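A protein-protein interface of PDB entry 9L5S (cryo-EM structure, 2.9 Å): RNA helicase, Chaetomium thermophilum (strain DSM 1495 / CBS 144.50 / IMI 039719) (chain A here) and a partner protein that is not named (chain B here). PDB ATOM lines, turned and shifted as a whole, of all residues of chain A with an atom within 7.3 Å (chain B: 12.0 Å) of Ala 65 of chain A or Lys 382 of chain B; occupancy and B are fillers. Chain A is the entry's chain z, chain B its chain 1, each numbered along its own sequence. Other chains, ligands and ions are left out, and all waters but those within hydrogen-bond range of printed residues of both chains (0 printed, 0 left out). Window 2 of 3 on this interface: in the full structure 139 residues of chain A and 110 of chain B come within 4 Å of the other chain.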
ATOM      1  N   LEU A  58      -5.555   0.220   8.673  1.00  0.00           N
ATOM      2  CA  LEU A  58      -5.438  -0.540   9.914  1.00  0.00           C
ATOM      3  C   LEU A  58      -4.049  -0.395  10.526  1.00  0.00           C
ATOM      4  O   LEU A  58      -3.909  -0.365  11.755  1.00  0.00           O
ATOM      5  CB  LEU A  58      -5.763  -2.013   9.663  1.00  0.00           C
ATOM      6  CG  LEU A  58      -7.214  -2.344   9.308  1.00  0.00           C
ATOM      7  CD1 LEU A  58      -7.380  -3.833   9.049  1.00  0.00           C
ATOM      8  CD2 LEU A  58      -8.151  -1.879  10.410  1.00  0.00           C
ATOM      9  N   GLU A  59      -3.012  -0.316   9.688  1.00  0.00           N
ATOM     10  CA  GLU A  59      -1.660  -0.114  10.202  1.00  0.00           C
ATOM     11  C   GLU A  59      -1.494   1.282  10.791  1.00  0.00           C
ATOM     12  O   GLU A  59      -0.806   1.456  11.804  1.00  0.00           O
ATOM     13  CB  GLU A  59      -0.635  -0.355   9.095  1.00  0.00           C
ATOM     14  CG  GLU A  59       0.773  -0.628   9.601  1.00  0.00           C
ATOM     15  CD  GLU A  59       1.615   0.630   9.688  1.00  0.00           C
ATOM     16  OE1 GLU A  59       1.337   1.586   8.934  1.00  0.00           O
ATOM     17  OE2 GLU A  59       2.554   0.663  10.512  1.00  0.00           O
ATOM     18  N   LYS A  60      -2.115   2.288  10.173  1.00  0.00           N
ATOM     19  CA  LYS A  60      -2.052   3.646  10.696  1.00  0.00           C
ATOM     20  C   LYS A  60      -2.989   3.873  11.875  1.00  0.00           C
ATOM     21  O   LYS A  60      -2.887   4.915  12.533  1.00  0.00           O
ATOM     22  CB  LYS A  60      -2.367   4.656   9.588  1.00  0.00           C
ATOM     23  CG  LYS A  60      -1.287   4.766   8.523  1.00  0.00           C
ATOM     24  CD  LYS A  60      -1.859   5.262   7.204  1.00  0.00           C
ATOM     25  CE  LYS A  60      -0.755   5.566   6.204  1.00  0.00           C
ATOM     26  NZ  LYS A  60      -1.030   4.961   4.871  1.00  0.00           N
ATOM     27  N   ALA A  61      -3.892   2.936  12.157  1.00  0.00           N
ATOM     28  CA  ALA A  61      -4.793   3.049  13.297  1.00  0.00           C
ATOM     29  C   ALA A  61      -4.180   2.535  14.592  1.00  0.00           C
ATOM     30  O   ALA A  61      -4.837   2.600  15.637  1.00  0.00           O
ATOM     31  CB  ALA A  61      -6.098   2.300  13.014  1.00  0.00           C
ATOM     32  N   GLY A  62      -2.950   2.030  14.553  1.00  0.00           N
ATOM     33  CA  GLY A  62      -2.304   1.518  15.744  1.00  0.00           C
ATOM     34  C   GLY A  62      -2.532   0.053  16.026  1.00  0.00           C
ATOM     35  O   GLY A  62      -2.289  -0.389  17.155  1.00  0.00           O
ATOM     36  N   TRP A  63      -2.983  -0.721  15.039  1.00  0.00           N
ATOM     37  CA  TRP A  63      -3.252  -2.137  15.247  1.00  0.00           C
ATOM     38  C   TRP A  63      -1.998  -2.999  15.191  1.00  0.00           C
ATOM     39  O   TRP A  63      -2.082  -4.199  15.475  1.00  0.00           O
ATOM     40  CB  TRP A  63      -4.268  -2.633  14.217  1.00  0.00           C
ATOM     41  CG  TRP A  63      -5.676  -2.271  14.567  1.00  0.00           C
ATOM     42  CD1 TRP A  63      -6.311  -1.093  14.303  1.00  0.00           C
ATOM     43  CD2 TRP A  63      -6.622  -3.089  15.264  1.00  0.00           C
ATOM     44  NE1 TRP A  63      -7.596  -1.129  14.786  1.00  0.00           N
ATOM     45  CE2 TRP A  63      -7.812  -2.344  15.381  1.00  0.00           C
ATOM     46  CE3 TRP A  63      -6.580  -4.382  15.797  1.00  0.00           C
ATOM     47  CZ2 TRP A  63      -8.948  -2.847  16.009  1.00  0.00           C
ATOM     48  CZ3 TRP A  63      -7.710  -4.880  16.420  1.00  0.00           C
ATOM     49  CH2 TRP A  63      -8.876  -4.114  16.521  1.00  0.00           C
ATOM     50  N   CYS A  64      -0.849  -2.428  14.833  1.00  0.00           N
ATOM     51  CA  CYS A  64       0.414  -3.156  14.807  1.00  0.00           C
ATOM     52  C   CYS A  64       1.409  -2.636  15.835  1.00  0.00           C
ATOM     53  O   CYS A  64       2.578  -3.034  15.808  1.00  0.00           O
ATOM     54  CB  CYS A  64       1.030  -3.099  13.409  1.00  0.00           C
ATOM     55  SG  CYS A  64      -0.060  -3.678  12.098  1.00  0.00           S
ATOM     56  N   ALA A  65       0.976  -1.752  16.739  1.00  0.00           N
ATOM     57  CA  ALA A  65       1.883  -1.228  17.753  1.00  0.00           C
ATOM     58  C   ALA A  65       2.204  -2.268  18.817  1.00  0.00           C
ATOM     59  O   ALA A  65       3.263  -2.199  19.450  1.00  0.00           O
ATOM     60  CB  ALA A  65       1.285   0.024  18.397  1.00  0.00           C
ATOM     61  N   ASP A  66       1.309  -3.237  19.028  1.00  0.00           N
ATOM     62  CA  ASP A  66       1.506  -4.291  20.015  1.00  0.00           C
ATOM     63  C   ASP A  66       2.123  -5.550  19.416  1.00  0.00           C
ATOM     64  O   ASP A  66       1.909  -6.652  19.940  1.00  0.00           O
ATOM     65  CB  ASP A  66       0.180  -4.623  20.701  1.00  0.00           C
ATOM     66  CG  ASP A  66      -0.972  -4.732  19.720  1.00  0.00           C
ATOM     67  OD1 ASP A  66      -0.799  -4.336  18.548  1.00  0.00           O
ATOM     68  OD2 ASP A  66      -2.050  -5.219  20.120  1.00  0.00           O
ATOM     69  N   GLY A  67       2.883  -5.417  18.331  1.00  0.00           N
ATOM     70  CA  GLY A  67       3.494  -6.572  17.701  1.00  0.00           C
ATOM     71  C   GLY A  67       2.526  -7.469  16.966  1.00  0.00           C
ATOM     72  O   GLY A  67       2.815  -8.654  16.770  1.00  0.00           O
ATOM     73  N   LYS A  68       1.380  -6.936  16.552  1.00  0.00           N
ATOM     74  CA  LYS A  68       0.369  -7.702  15.845  1.00  0.00           C
ATOM     75  C   LYS A  68       0.571  -7.570  14.337  1.00  0.00           C
ATOM     76  O   LYS A  68       1.425  -6.820  13.858  1.00  0.00           O
ATOM     77  CB  LYS A  68      -1.029  -7.248  16.263  1.00  0.00           C
ATOM     78  CG  LYS A  68      -1.403  -7.631  17.686  1.00  0.00           C
ATOM     79  CD  LYS A  68      -1.493  -9.141  17.841  1.00  0.00           C
ATOM     80  CE  LYS A  68      -1.927  -9.529  19.245  1.00  0.00           C
ATOM     81  NZ  LYS A  68      -1.937 -11.005  19.434  1.00  0.00           N
ATOM     82  N   ARG A 114       4.457  -5.728   8.931  1.00  0.00           N
ATOM     83  CA  ARG A 114       3.176  -5.576   9.610  1.00  0.00           C
ATOM     84  C   ARG A 114       1.990  -5.917   8.725  1.00  0.00           C
ATOM     85  O   ARG A 114       1.069  -6.605   9.174  1.00  0.00           O
ATOM     86  CB  ARG A 114       3.026  -4.142  10.137  1.00  0.00           C
ATOM     87  CG  ARG A 114       4.169  -3.691  11.031  1.00  0.00           C
ATOM     88  CD  ARG A 114       4.038  -2.223  11.399  1.00  0.00           C
ATOM     89  NE  ARG A 114       5.244  -1.713  12.040  1.00  0.00           N
ATOM     90  CZ  ARG A 114       5.498  -0.427  12.242  1.00  0.00           C
ATOM     91  NH1 ARG A 114       4.648   0.513  11.864  1.00  0.00           N
ATOM     92  NH2 ARG A 114       6.633  -0.076  12.840  1.00  0.00           N
ATOM     93  N   GLY B 376     -16.870  11.388  20.908  1.00  0.00           N
ATOM     94  CA  GLY B 376     -16.627  10.824  22.221  1.00  0.00           C
ATOM     95  C   GLY B 376     -15.891   9.502  22.160  1.00  0.00           C
ATOM     96  O   GLY B 376     -15.192   9.128  23.106  1.00  0.00           O
ATOM     97  N   TRP B 377     -16.043   8.785  21.050  1.00  0.00           N
ATOM     98  CA  TRP B 377     -15.313   7.540  20.860  1.00  0.00           C
ATOM     99  C   TRP B 377     -13.864   7.827  20.487  1.00  0.00           C
ATOM    100  O   TRP B 377     -13.574   8.744  19.713  1.00  0.00           O
ATOM    101  CB  TRP B 377     -15.978   6.691  19.778  1.00  0.00           C
ATOM    102  CG  TRP B 377     -15.321   5.359  19.571  1.00  0.00           C
ATOM    103  CD1 TRP B 377     -14.478   5.011  18.557  1.00  0.00           C
ATOM    104  CD2 TRP B 377     -15.451   4.199  20.402  1.00  0.00           C
ATOM    105  NE1 TRP B 377     -14.076   3.706  18.703  1.00  0.00           N
ATOM    106  CE2 TRP B 377     -14.659   3.184  19.827  1.00  0.00           C
ATOM    107  CE3 TRP B 377     -16.159   3.918  21.574  1.00  0.00           C
ATOM    108  CZ2 TRP B 377     -14.556   1.911  20.385  1.00  0.00           C
ATOM    109  CZ3 TRP B 377     -16.056   2.654  22.127  1.00  0.00           C
ATOM    110  CH2 TRP B 377     -15.260   1.666  21.532  1.00  0.00           C
ATOM    111  N   VAL B 378     -12.951   7.036  21.044  1.00  0.00           N
ATOM    112  CA  VAL B 378     -11.521   7.203  20.824  1.00  0.00           C
ATOM    113  C   VAL B 378     -10.920   5.837  20.509  1.00  0.00           C
ATOM    114  O   VAL B 378     -11.388   4.809  21.014  1.00  0.00           O
ATOM    115  CB  VAL B 378     -10.839   7.873  22.043  1.00  0.00           C
ATOM    116  CG1 VAL B 378     -10.927   6.997  23.295  1.00  0.00           C
ATOM    117  CG2 VAL B 378      -9.394   8.271  21.738  1.00  0.00           C
ATOM    118  N   SER B 379      -9.921   5.821  19.628  1.00  0.00           N
ATOM    119  CA  SER B 379      -9.217   4.585  19.308  1.00  0.00           C
ATOM    120  C   SER B 379      -8.357   4.167  20.495  1.00  0.00           C
ATOM    121  O   SER B 379      -7.501   4.933  20.950  1.00  0.00           O
ATOM    122  CB  SER B 379      -8.361   4.772  18.058  1.00  0.00           C
ATOM    123  OG  SER B 379      -7.305   5.686  18.295  1.00  0.00           O
ATOM    124  N   SER B 380      -8.591   2.954  21.000  1.00  0.00           N
ATOM    125  CA  SER B 380      -7.861   2.486  22.175  1.00  0.00           C
ATOM    126  C   SER B 380      -6.405   2.180  21.844  1.00  0.00           C
ATOM    127  O   SER B 380      -5.512   2.428  22.662  1.00  0.00           O
ATOM    128  CB  SER B 380      -8.548   1.253  22.762  1.00  0.00           C
ATOM    129  OG  SER B 380      -9.868   1.556  23.181  1.00  0.00           O
ATOM    130  N   LYS B 381      -6.146   1.644  20.654  1.00  0.00           N
ATOM    131  CA  LYS B 381      -4.796   1.247  20.260  1.00  0.00           C
ATOM    132  C   LYS B 381      -4.047   2.474  19.757  1.00  0.00           C
ATOM    133  O   LYS B 381      -4.293   2.961  18.651  1.00  0.00           O
ATOM    134  CB  LYS B 381      -4.852   0.154  19.200  1.00  0.00           C
ATOM    135  CG  LYS B 381      -5.256  -1.208  19.743  1.00  0.00           C
ATOM    136  CD  LYS B 381      -5.151  -2.286  18.680  1.00  0.00           C
ATOM    137  CE  LYS B 381      -5.609  -3.633  19.217  1.00  0.00           C
ATOM    138  NZ  LYS B 381      -4.675  -4.167  20.245  1.00  0.00           N
ATOM    139  N   LYS B 382      -3.129   2.980  20.577  1.00  0.00           N
ATOM    140  CA  LYS B 382      -2.312   4.117  20.176  1.00  0.00           C
ATOM    141  C   LYS B 382      -1.301   3.692  19.111  1.00  0.00           C
ATOM    142  O   LYS B 382      -0.703   2.618  19.215  1.00  0.00           O
ATOM    143  CB  LYS B 382      -1.579   4.706  21.384  1.00  0.00           C
ATOM    144  CG  LYS B 382      -2.447   5.245  22.539  1.00  0.00           C
ATOM    145  CD  LYS B 382      -3.205   6.549  22.221  1.00  0.00           C
ATOM    146  CE  LYS B 382      -4.631   6.337  21.717  1.00  0.00           C
ATOM    147  NZ  LYS B 382      -5.353   7.626  21.527  1.00  0.00           N
ATOM    148  N   PRO B 383      -1.088   4.515  18.072  1.00  0.00           N
ATOM    149  CA  PRO B 383      -0.099   4.209  17.034  1.00  0.00           C
ATOM    150  C   PRO B 383       1.333   4.458  17.498  1.00  0.00           C
ATOM    151  O   PRO B 383       1.522   5.091  18.537  1.00  0.00           O
ATOM    152  CB  PRO B 383      -0.478   5.163  15.901  1.00  0.00           C
ATOM    153  CG  PRO B 383      -1.102   6.323  16.591  1.00  0.00           C
ATOM    154  CD  PRO B 383      -1.814   5.768  17.794  1.00  0.00           C
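Of chain B, only Lys 381 (3.3 Å), Lys 382 (3.98 Å) and Pro 383 (3.7 Å) come within 4 Å of Gly 62 of chain A.
Printed residues of chain B within 4 Å of Trp 63 of chain A: Lys 381.
No residue of chain B comes within 4 Å of Cys 64 of chain A.
Of the printed residues of chain B, Ala 65 of chain A touches Lys 382 (3.4 Å).
No residue of chain B comes within 4 Å of Gly 67 of chain A.
Ser 379 of chain B touches none of the printed residues of chain A.
Printed residues of chain A within 4 Å of Lys 381 of chain B: Ala 61, Gly 62, Trp 63 and Asp 66.
Lys 382 of chain B touches just these residues of chain A: Gly 62 (3.98 Å) and Ala 65 (3.4 Å).
Printed residues of chain A within 4 Å of Pro 383 of chain B: Gly 62.
The nearest residue of chain B that does not touch Ala 65 of chain A is Pro 383 of chain B (4.5 Å).
The nearest printed residue of chain B that does not touch Trp 63 of chain A is Lys 382 of chain B (5.8 Å).
The backbone carbonyl oxygen (O) of Ser 379 of chain B sits close to the side-chain amino group (NZ) of Lys 382 of chain B (3.5 Å).
The backbone carbonyl oxygen of Leu 58 of chain A lies close to the backbone NH of Trp 63 of chain A (3.4 Å).
Among the printed residues, pairs that only touch across the chains: Gly 62 of chain A with Lys 381 of chain B (3.3 Å), Ala 65 of chain A with Lys 382 of chain B (3.4 Å), Trp 63 of chain A with Lys 381 of chain B (3.6 Å), Gly 62 of chain A with Pro 383 of chain B (3.7 Å) and Gly 62 of chain A with Lys 382 of chain B (3.98 Å).
O of Ala 61 of chain A lies close to O of Lys 381 of chain B (3.1 Å).
The side-chain carboxylate (OD2) of Asp 66 of chain A lies within salt-bridge range of the side-chain amino group (NZ) of Lys 381 of chain B (2.8 Å).
Printed residues of chain B that touch a printed residue of chain A: Lys 381, Lys 382 and Pro 383.
Printed residues of chain A that touch a printed residue of chain B: Ala 61, Gly 62, Trp 63, Ala 65 and Asp 66.
Hydrophobic or aromatic side chains of chain A that line the printed part of chain B: Trp 63 and Ala 65.
Along chain A the printed residues that touch a printed residue of chain B span positions 61 to 66.
Among the printed residues, 7 pairs touch across the chains.
Among the printed residues, Asp or Glu carboxylates within 4 Å of a Lys or Arg side-chain nitrogen of the other chain: Asp 66 of chain A with Lys 381 of chain B.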
